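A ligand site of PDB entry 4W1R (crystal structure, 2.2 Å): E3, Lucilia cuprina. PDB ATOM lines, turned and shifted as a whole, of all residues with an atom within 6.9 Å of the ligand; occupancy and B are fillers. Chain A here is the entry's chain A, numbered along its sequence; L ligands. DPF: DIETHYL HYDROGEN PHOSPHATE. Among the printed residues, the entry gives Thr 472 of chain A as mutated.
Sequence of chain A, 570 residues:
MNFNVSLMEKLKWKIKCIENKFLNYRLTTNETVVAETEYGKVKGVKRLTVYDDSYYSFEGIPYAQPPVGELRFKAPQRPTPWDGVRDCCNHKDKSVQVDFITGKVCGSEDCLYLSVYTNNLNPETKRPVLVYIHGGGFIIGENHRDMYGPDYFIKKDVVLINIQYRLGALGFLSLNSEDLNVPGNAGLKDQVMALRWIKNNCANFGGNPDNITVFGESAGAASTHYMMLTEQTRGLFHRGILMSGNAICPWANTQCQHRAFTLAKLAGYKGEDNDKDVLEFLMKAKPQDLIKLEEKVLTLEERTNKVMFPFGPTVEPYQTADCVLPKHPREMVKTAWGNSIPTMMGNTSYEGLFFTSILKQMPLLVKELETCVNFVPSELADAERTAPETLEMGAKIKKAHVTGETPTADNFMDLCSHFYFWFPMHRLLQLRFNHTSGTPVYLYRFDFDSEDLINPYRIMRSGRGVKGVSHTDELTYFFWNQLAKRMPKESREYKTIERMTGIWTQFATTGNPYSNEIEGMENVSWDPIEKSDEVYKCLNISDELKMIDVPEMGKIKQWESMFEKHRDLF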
ATOM      1  N   HIS A 134      -7.460 -13.590  -4.767  1.00  0.00           N
ATOM      2  CA  HIS A 134      -7.476 -13.972  -3.355  1.00  0.00           C
ATOM      3  C   HIS A 134      -6.856 -15.362  -3.115  1.00  0.00           C
ATOM      4  O   HIS A 134      -6.809 -16.201  -4.002  1.00  0.00           O
ATOM      5  CB  HIS A 134      -8.896 -13.932  -2.809  1.00  0.00           C
ATOM      6  CG  HIS A 134      -9.792 -15.008  -3.356  1.00  0.00           C
ATOM      7  ND1 HIS A 134      -9.822 -16.291  -2.848  1.00  0.00           N
ATOM      8  CD2 HIS A 134     -10.697 -14.983  -4.364  1.00  0.00           C
ATOM      9  CE1 HIS A 134     -10.711 -17.001  -3.515  1.00  0.00           C
ATOM     10  NE2 HIS A 134     -11.260 -16.234  -4.441  1.00  0.00           N
ATOM     11  N   GLY A 135      -6.363 -15.581  -1.899  1.00  0.00           N
ATOM     12  CA  GLY A 135      -5.874 -16.881  -1.510  1.00  0.00           C
ATOM     13  C   GLY A 135      -6.994 -17.669  -0.878  1.00  0.00           C
ATOM     14  O   GLY A 135      -8.168 -17.328  -1.076  1.00  0.00           O
ATOM     15  N   GLY A 136      -6.643 -18.698  -0.124  1.00  0.00           N
ATOM     16  CA  GLY A 136      -7.614 -19.598   0.468  1.00  0.00           C
ATOM     17  C   GLY A 136      -7.433 -21.030  -0.011  1.00  0.00           C
ATOM     18  O   GLY A 136      -8.413 -21.781  -0.136  1.00  0.00           O
ATOM     19  N   GLY A 137      -6.188 -21.391  -0.283  1.00  0.00           N
ATOM     20  CA  GLY A 137      -5.798 -22.764  -0.579  1.00  0.00           C
ATOM     21  C   GLY A 137      -6.513 -23.397  -1.756  1.00  0.00           C
ATOM     22  O   GLY A 137      -6.522 -24.620  -1.877  1.00  0.00           O
ATOM     23  N   PHE A 138      -7.101 -22.560  -2.600  1.00  0.00           N
ATOM     24  CA  PHE A 138      -7.870 -22.956  -3.773  1.00  0.00           C
ATOM     25  C   PHE A 138      -9.191 -23.617  -3.399  1.00  0.00           C
ATOM     26  O   PHE A 138      -9.875 -24.147  -4.260  1.00  0.00           O
ATOM     27  CB  PHE A 138      -7.065 -23.887  -4.687  1.00  0.00           C
ATOM     28  CG  PHE A 138      -5.835 -23.258  -5.284  1.00  0.00           C
ATOM     29  CD1 PHE A 138      -5.947 -22.261  -6.232  1.00  0.00           C
ATOM     30  CD2 PHE A 138      -4.567 -23.689  -4.900  1.00  0.00           C
ATOM     31  CE1 PHE A 138      -4.806 -21.681  -6.793  1.00  0.00           C
ATOM     32  CE2 PHE A 138      -3.423 -23.118  -5.462  1.00  0.00           C
ATOM     33  CZ  PHE A 138      -3.548 -22.115  -6.409  1.00  0.00           C
ATOM     34  N   ILE A 140     -11.292 -22.045  -0.415  1.00  0.00           N
ATOM     35  CA  ILE A 140     -12.169 -20.985   0.115  1.00  0.00           C
ATOM     36  C   ILE A 140     -11.791 -19.626  -0.474  1.00  0.00           C
ATOM     37  O   ILE A 140     -10.747 -19.507  -1.137  1.00  0.00           O
ATOM     38  CB  ILE A 140     -12.124 -20.871   1.675  1.00  0.00           C
ATOM     39  CG1 ILE A 140     -10.721 -20.480   2.150  1.00  0.00           C
ATOM     40  CG2 ILE A 140     -12.631 -22.142   2.362  1.00  0.00           C
ATOM     41  CD1 ILE A 140     -10.714 -19.783   3.460  1.00  0.00           C
ATOM     42  N   GLU A 217      -2.040 -13.209  -2.643  1.00  0.00           N
ATOM     43  CA  GLU A 217      -1.421 -13.712  -1.440  1.00  0.00           C
ATOM     44  C   GLU A 217      -1.796 -15.206  -1.233  1.00  0.00           C
ATOM     45  O   GLU A 217      -2.894 -15.590  -1.576  1.00  0.00           O
ATOM     46  CB  GLU A 217      -1.869 -12.840  -0.263  1.00  0.00           C
ATOM     47  CG  GLU A 217      -1.092 -13.025   1.000  1.00  0.00           C
ATOM     48  CD  GLU A 217      -1.891 -13.779   2.041  1.00  0.00           C
ATOM     49  OE1 GLU A 217      -3.113 -13.948   1.824  1.00  0.00           O
ATOM     50  OE2 GLU A 217      -1.286 -14.205   3.053  1.00  0.00           O
ATOM     51  N   SER A 218      -0.863 -16.035  -0.743  1.00  0.00           N
ATOM     52  CA  SER A 218      -1.107 -17.480  -0.463  1.00  0.00           C
ATOM     53  C   SER A 218      -1.385 -18.313  -1.752  1.00  0.00           C
ATOM     54  O   SER A 218      -0.558 -18.343  -2.662  1.00  0.00           O
ATOM     55  CB  SER A 218      -2.269 -17.618   0.535  1.00  0.00           C
ATOM     56  OG  SER A 218      -2.429 -18.955   1.009  1.00  0.00           O
ATOM     57  N   ALA A 219      -2.550 -18.967  -1.827  1.00  0.00           N
ATOM     58  CA  ALA A 219      -3.016 -19.550  -3.086  1.00  0.00           C
ATOM     59  C   ALA A 219      -3.186 -18.473  -4.142  1.00  0.00           C
ATOM     60  O   ALA A 219      -3.112 -18.761  -5.327  1.00  0.00           O
ATOM     61  CB  ALA A 219      -4.354 -20.298  -2.896  1.00  0.00           C
ATOM     62  N   GLY A 220      -3.436 -17.230  -3.718  1.00  0.00           N
ATOM     63  CA  GLY A 220      -3.500 -16.102  -4.639  1.00  0.00           C
ATOM     64  C   GLY A 220      -2.130 -15.742  -5.177  1.00  0.00           C
ATOM     65  O   GLY A 220      -1.979 -15.306  -6.333  1.00  0.00           O
ATOM     66  N   ALA A 221      -1.110 -15.955  -4.350  1.00  0.00           N
ATOM     67  CA  ALA A 221       0.271 -15.777  -4.794  1.00  0.00           C
ATOM     68  C   ALA A 221       0.647 -16.841  -5.803  1.00  0.00           C
ATOM     69  O   ALA A 221       1.265 -16.526  -6.809  1.00  0.00           O
ATOM     70  CB  ALA A 221       1.225 -15.800  -3.605  1.00  0.00           C
ATOM     71  N   SER A 244       3.773 -14.097  -0.134  1.00  0.00           N
ATOM     72  CA  SER A 244       3.764 -15.393   0.584  1.00  0.00           C
ATOM     73  C   SER A 244       3.321 -16.552  -0.302  1.00  0.00           C
ATOM     74  O   SER A 244       2.311 -17.214  -0.019  1.00  0.00           O
ATOM     75  CB  SER A 244       2.844 -15.360   1.820  1.00  0.00           C
ATOM     76  OG  SER A 244       3.251 -14.395   2.761  1.00  0.00           O
ATOM     77  N   TRP A 251       2.385 -27.164  -1.445  1.00  0.00           N
ATOM     78  CA  TRP A 251       0.918 -27.139  -1.486  1.00  0.00           C
ATOM     79  C   TRP A 251       0.295 -26.618  -2.808  1.00  0.00           C
ATOM     80  O   TRP A 251      -0.922 -26.714  -3.005  1.00  0.00           O
ATOM     81  CB  TRP A 251       0.391 -26.281  -0.329  1.00  0.00           C
ATOM     82  CG  TRP A 251       1.070 -24.967  -0.247  1.00  0.00           C
ATOM     83  CD1 TRP A 251       2.185 -24.679   0.485  1.00  0.00           C
ATOM     84  CD2 TRP A 251       0.721 -23.773  -0.948  1.00  0.00           C
ATOM     85  NE1 TRP A 251       2.550 -23.364   0.294  1.00  0.00           N
ATOM     86  CE2 TRP A 251       1.662 -22.782  -0.586  1.00  0.00           C
ATOM     87  CE3 TRP A 251      -0.302 -23.432  -1.847  1.00  0.00           C
ATOM     88  CZ2 TRP A 251       1.629 -21.469  -1.088  1.00  0.00           C
ATOM     89  CZ3 TRP A 251      -0.347 -22.115  -2.338  1.00  0.00           C
ATOM     90  CH2 TRP A 251       0.617 -21.160  -1.962  1.00  0.00           C
ATOM     91  N   ALA A 252       1.114 -26.072  -3.707  1.00  0.00           N
ATOM     92  CA  ALA A 252       0.587 -25.296  -4.854  1.00  0.00           C
ATOM     93  C   ALA A 252       0.261 -26.144  -6.084  1.00  0.00           C
ATOM     94  O   ALA A 252      -0.270 -25.631  -7.066  1.00  0.00           O
ATOM     95  CB  ALA A 252       1.567 -24.197  -5.247  1.00  0.00           C
ATOM     96  N   MET A 308      -1.716 -31.186   1.344  1.00  0.00           N
ATOM     97  CA  MET A 308      -2.588 -30.326   2.139  1.00  0.00           C
ATOM     98  C   MET A 308      -4.040 -30.377   1.653  1.00  0.00           C
ATOM     99  O   MET A 308      -4.968 -30.445   2.471  1.00  0.00           O
ATOM    100  CB  MET A 308      -2.049 -28.888   2.131  1.00  0.00           C
ATOM    101  CG  MET A 308      -2.487 -28.072   3.351  1.00  0.00           C
ATOM    102  SD  MET A 308      -1.980 -26.339   3.305  1.00  0.00           S
ATOM    103  CE  MET A 308      -0.270 -26.471   3.787  1.00  0.00           C
ATOM    104  N   PHE A 309      -4.228 -30.376   0.335  1.00  0.00           N
ATOM    105  CA  PHE A 309      -5.553 -30.330  -0.273  1.00  0.00           C
ATOM    106  C   PHE A 309      -5.741 -31.421  -1.339  1.00  0.00           C
ATOM    107  O   PHE A 309      -4.823 -31.677  -2.111  1.00  0.00           O
ATOM    108  CB  PHE A 309      -5.798 -28.955  -0.921  1.00  0.00           C
ATOM    109  CG  PHE A 309      -5.432 -27.788  -0.062  1.00  0.00           C
ATOM    110  CD1 PHE A 309      -6.279 -27.360   0.954  1.00  0.00           C
ATOM    111  CD2 PHE A 309      -4.250 -27.105  -0.277  1.00  0.00           C
ATOM    112  CE1 PHE A 309      -5.956 -26.274   1.743  1.00  0.00           C
ATOM    113  CE2 PHE A 309      -3.916 -25.995   0.525  1.00  0.00           C
ATOM    114  CZ  PHE A 309      -4.787 -25.587   1.539  1.00  0.00           C
ATOM    115  N   PHE A 354       0.981 -19.191  11.900  1.00  0.00           N
ATOM    116  CA  PHE A 354      -0.349 -19.549  11.458  1.00  0.00           C
ATOM    117  C   PHE A 354      -0.826 -20.897  12.022  1.00  0.00           C
ATOM    118  O   PHE A 354      -1.972 -21.046  12.421  1.00  0.00           O
ATOM    119  CB  PHE A 354      -0.348 -19.585   9.927  1.00  0.00           C
ATOM    120  CG  PHE A 354      -1.672 -19.894   9.320  1.00  0.00           C
ATOM    121  CD1 PHE A 354      -2.040 -21.205   9.047  1.00  0.00           C
ATOM    122  CD2 PHE A 354      -2.570 -18.878   9.026  1.00  0.00           C
ATOM    123  CE1 PHE A 354      -3.277 -21.490   8.491  1.00  0.00           C
ATOM    124  CE2 PHE A 354      -3.811 -19.154   8.471  1.00  0.00           C
ATOM    125  CZ  PHE A 354      -4.160 -20.459   8.208  1.00  0.00           C
ATOM    126  N   PHE A 355       0.064 -21.877  12.058  1.00  0.00           N
ATOM    127  CA  PHE A 355      -0.299 -23.261  12.351  1.00  0.00           C
ATOM    128  C   PHE A 355      -0.556 -23.567  13.811  1.00  0.00           C
ATOM    129  O   PHE A 355      -0.703 -24.730  14.168  1.00  0.00           O
ATOM    130  CB  PHE A 355       0.801 -24.204  11.870  1.00  0.00           C
ATOM    131  CG  PHE A 355       0.905 -24.294  10.379  1.00  0.00           C
ATOM    132  CD1 PHE A 355       0.175 -25.233   9.685  1.00  0.00           C
ATOM    133  CD2 PHE A 355       1.716 -23.416   9.678  1.00  0.00           C
ATOM    134  CE1 PHE A 355       0.254 -25.317   8.307  1.00  0.00           C
ATOM    135  CE2 PHE A 355       1.804 -23.497   8.300  1.00  0.00           C
ATOM    136  CZ  PHE A 355       1.078 -24.446   7.615  1.00  0.00           C
ATOM    137  N   TYR A 420       6.878 -24.410   3.788  1.00  0.00           N
ATOM    138  CA  TYR A 420       5.808 -23.913   2.953  1.00  0.00           C
ATOM    139  C   TYR A 420       6.132 -22.605   2.216  1.00  0.00           C
ATOM    140  O   TYR A 420       5.530 -22.357   1.179  1.00  0.00           O
ATOM    141  CB  TYR A 420       4.524 -23.737   3.786  1.00  0.00           C
ATOM    142  CG  TYR A 420       3.988 -25.039   4.328  1.00  0.00           C
ATOM    143  CD1 TYR A 420       3.442 -26.005   3.482  1.00  0.00           C
ATOM    144  CD2 TYR A 420       4.002 -25.295   5.695  1.00  0.00           C
ATOM    145  CE1 TYR A 420       2.946 -27.210   3.976  1.00  0.00           C
ATOM    146  CE2 TYR A 420       3.507 -26.503   6.209  1.00  0.00           C
ATOM    147  CZ  TYR A 420       2.975 -27.449   5.335  1.00  0.00           C
ATOM    148  OH  TYR A 420       2.482 -28.633   5.842  1.00  0.00           O
ATOM    149  N   PHE A 421       7.085 -21.799   2.693  1.00  0.00           N
ATOM    150  CA  PHE A 421       7.308 -20.482   2.072  1.00  0.00           C
ATOM    151  C   PHE A 421       8.750 -20.067   1.701  1.00  0.00           C
ATOM    152  O   PHE A 421       9.020 -19.810   0.526  1.00  0.00           O
ATOM    153  CB  PHE A 421       6.694 -19.402   2.970  1.00  0.00           C
ATOM    154  CG  PHE A 421       5.232 -19.644   3.286  1.00  0.00           C
ATOM    155  CD1 PHE A 421       4.259 -19.406   2.340  1.00  0.00           C
ATOM    156  CD2 PHE A 421       4.848 -20.115   4.536  1.00  0.00           C
ATOM    157  CE1 PHE A 421       2.922 -19.640   2.622  1.00  0.00           C
ATOM    158  CE2 PHE A 421       3.506 -20.363   4.826  1.00  0.00           C
ATOM    159  CZ  PHE A 421       2.544 -20.128   3.859  1.00  0.00           C
ATOM    160  N   TYR A 457      -8.980 -13.984   9.097  1.00  0.00           N
ATOM    161  CA  TYR A 457      -8.092 -15.139   9.220  1.00  0.00           C
ATOM    162  C   TYR A 457      -7.504 -15.306  10.613  1.00  0.00           C
ATOM    163  O   TYR A 457      -7.040 -16.393  10.961  1.00  0.00           O
ATOM    164  CB  TYR A 457      -6.955 -15.051   8.206  1.00  0.00           C
ATOM    165  CG  TYR A 457      -7.362 -15.408   6.805  1.00  0.00           C
ATOM    166  CD1 TYR A 457      -7.453 -16.739   6.420  1.00  0.00           C
ATOM    167  CD2 TYR A 457      -7.637 -14.429   5.860  1.00  0.00           C
ATOM    168  CE1 TYR A 457      -7.810 -17.094   5.129  1.00  0.00           C
ATOM    169  CE2 TYR A 457      -8.000 -14.766   4.572  1.00  0.00           C
ATOM    170  CZ  TYR A 457      -8.082 -16.096   4.206  1.00  0.00           C
ATOM    171  OH  TYR A 457      -8.438 -16.453   2.925  1.00  0.00           O
ATOM    172  N   MET A 460      -9.597 -17.773  12.354  1.00  0.00           N
ATOM    173  CA  MET A 460      -9.340 -19.124  11.884  1.00  0.00           C
ATOM    174  C   MET A 460      -8.121 -19.757  12.555  1.00  0.00           C
ATOM    175  O   MET A 460      -8.219 -20.829  13.135  1.00  0.00           O
ATOM    176  CB  MET A 460      -9.153 -19.116  10.364  1.00  0.00           C
ATOM    177  CG  MET A 460      -8.903 -20.470   9.752  1.00  0.00           C
ATOM    178  SD  MET A 460      -8.446 -20.403   8.009  1.00  0.00           S
ATOM    179  CE  MET A 460      -9.892 -19.642   7.293  1.00  0.00           C
ATOM    180  N   HIS A 471       1.393 -15.451   8.612  1.00  0.00           N
ATOM    181  CA  HIS A 471       0.820 -15.501   7.270  1.00  0.00           C
ATOM    182  C   HIS A 471      -0.589 -14.880   7.280  1.00  0.00           C
ATOM    183  O   HIS A 471      -1.390 -15.213   8.168  1.00  0.00           O
ATOM    184  CB  HIS A 471       0.803 -16.974   6.791  1.00  0.00           C
ATOM    185  CG  HIS A 471       0.275 -17.175   5.416  1.00  0.00           C
ATOM    186  ND1 HIS A 471      -0.965 -17.733   5.165  1.00  0.00           N
ATOM    187  CD2 HIS A 471       0.799 -16.883   4.198  1.00  0.00           C
ATOM    188  CE1 HIS A 471      -1.176 -17.785   3.861  1.00  0.00           C
ATOM    189  NE2 HIS A 471      -0.126 -17.274   3.253  1.00  0.00           N
ATOM    190  N   THR A 472      -0.862 -13.966   6.336  1.00  0.00           N
ATOM    191  CA  THR A 472      -2.122 -13.190   6.182  1.00  0.00           C
ATOM    192  C   THR A 472      -2.317 -12.007   7.132  1.00  0.00           C
ATOM    193  O   THR A 472      -3.264 -11.241   6.956  1.00  0.00           O
ATOM    194  CB  THR A 472      -3.420 -14.046   6.335  1.00  0.00           C
ATOM    195  OG1 THR A 472      -3.642 -14.329   7.727  1.00  0.00           O
ATOM    196  CG2 THR A 472      -3.342 -15.326   5.527  1.00  0.00           C
ATOM    197  N   LEU A 475      -2.644  -8.641   5.088  1.00  0.00           N
ATOM    198  CA  LEU A 475      -3.857  -8.285   4.338  1.00  0.00           C
ATOM    199  C   LEU A 475      -4.631  -7.193   5.051  1.00  0.00           C
ATOM    200  O   LEU A 475      -5.409  -6.461   4.441  1.00  0.00           O
ATOM    201  CB  LEU A 475      -4.760  -9.504   4.145  1.00  0.00           C
ATOM    202  CG  LEU A 475      -4.220 -10.582   3.199  1.00  0.00           C
ATOM    203  CD1 LEU A 475      -5.211 -11.740   3.109  1.00  0.00           C
ATOM    204  CD2 LEU A 475      -3.910  -9.987   1.808  1.00  0.00           C
HETATM  205  O4  DPF L   1      -4.074 -19.612   0.495  1.00  0.00           O
HETATM  206  P1  DPF L   1      -3.431 -19.668   1.861  1.00  0.00           P
HETATM  207  O3  DPF L   1      -2.855 -21.224   2.018  1.00  0.00           O
HETATM  208  C1  DPF L   1      -1.726 -21.593   1.304  1.00  0.00           C
HETATM  209  C4  DPF L   1      -1.198 -22.895   1.873  1.00  0.00           C
HETATM  210  O1  DPF L   1      -4.737 -19.702   2.887  1.00  0.00           O
HETATM  211  C2  DPF L   1      -5.115 -18.526   3.509  1.00  0.00           C
HETATM  212  C3  DPF L   1      -4.511 -18.505   4.907  1.00  0.00           C
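Residues that only touch the ligand: Thr 472 (3.4 Å), Tyr 457 (3.5 Å), Trp 251 (3.5 Å), His 471 (3.6 Å), Phe 354 (3.7 Å), Gly 135 (3.8 Å) and Met 308 (3.8 Å). Hydrophobic or aromatic side chains within 4 Å of the ligand: Ala 219, Trp 251, Met 308, Phe 354, Tyr 457 and His 471.
OG of Ser 218 is bonded to P1 of the ligand (1.5 Å). The backbone NH of Gly 136 sits at hydrogen-bond distance from an oxygen (O4) of the ligand, 2.8 Å away. The backbone NH (N) of Ala 219 is in hydrogen-bond range of an oxygen (O4) of the ligand. The backbone NH (N) of Gly 137 sits at hydrogen-bond distance from an oxygen (O4) of the ligand.
The backbone carbonyl oxygen (O) of Ser 244 sits close to the backbone NH (N) of Ser 218, at 3.5 Å. The side-chain carboxylate (OE2) of Glu 217 sits at hydrogen-bond distance from the backbone NH (N) of Thr 472, 3.3 Å away. NE1 of Trp 251 lies within hydrogen-bond range of O of Tyr 420 (3.3 Å). A ring nitrogen (NE2) of His 471 sits at hydrogen-bond distance from the side-chain carboxylate (OE2) of Glu 217 (3.3 Å). O of Glu 217 sits close to N of Gly 135, at 3.5 Å.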
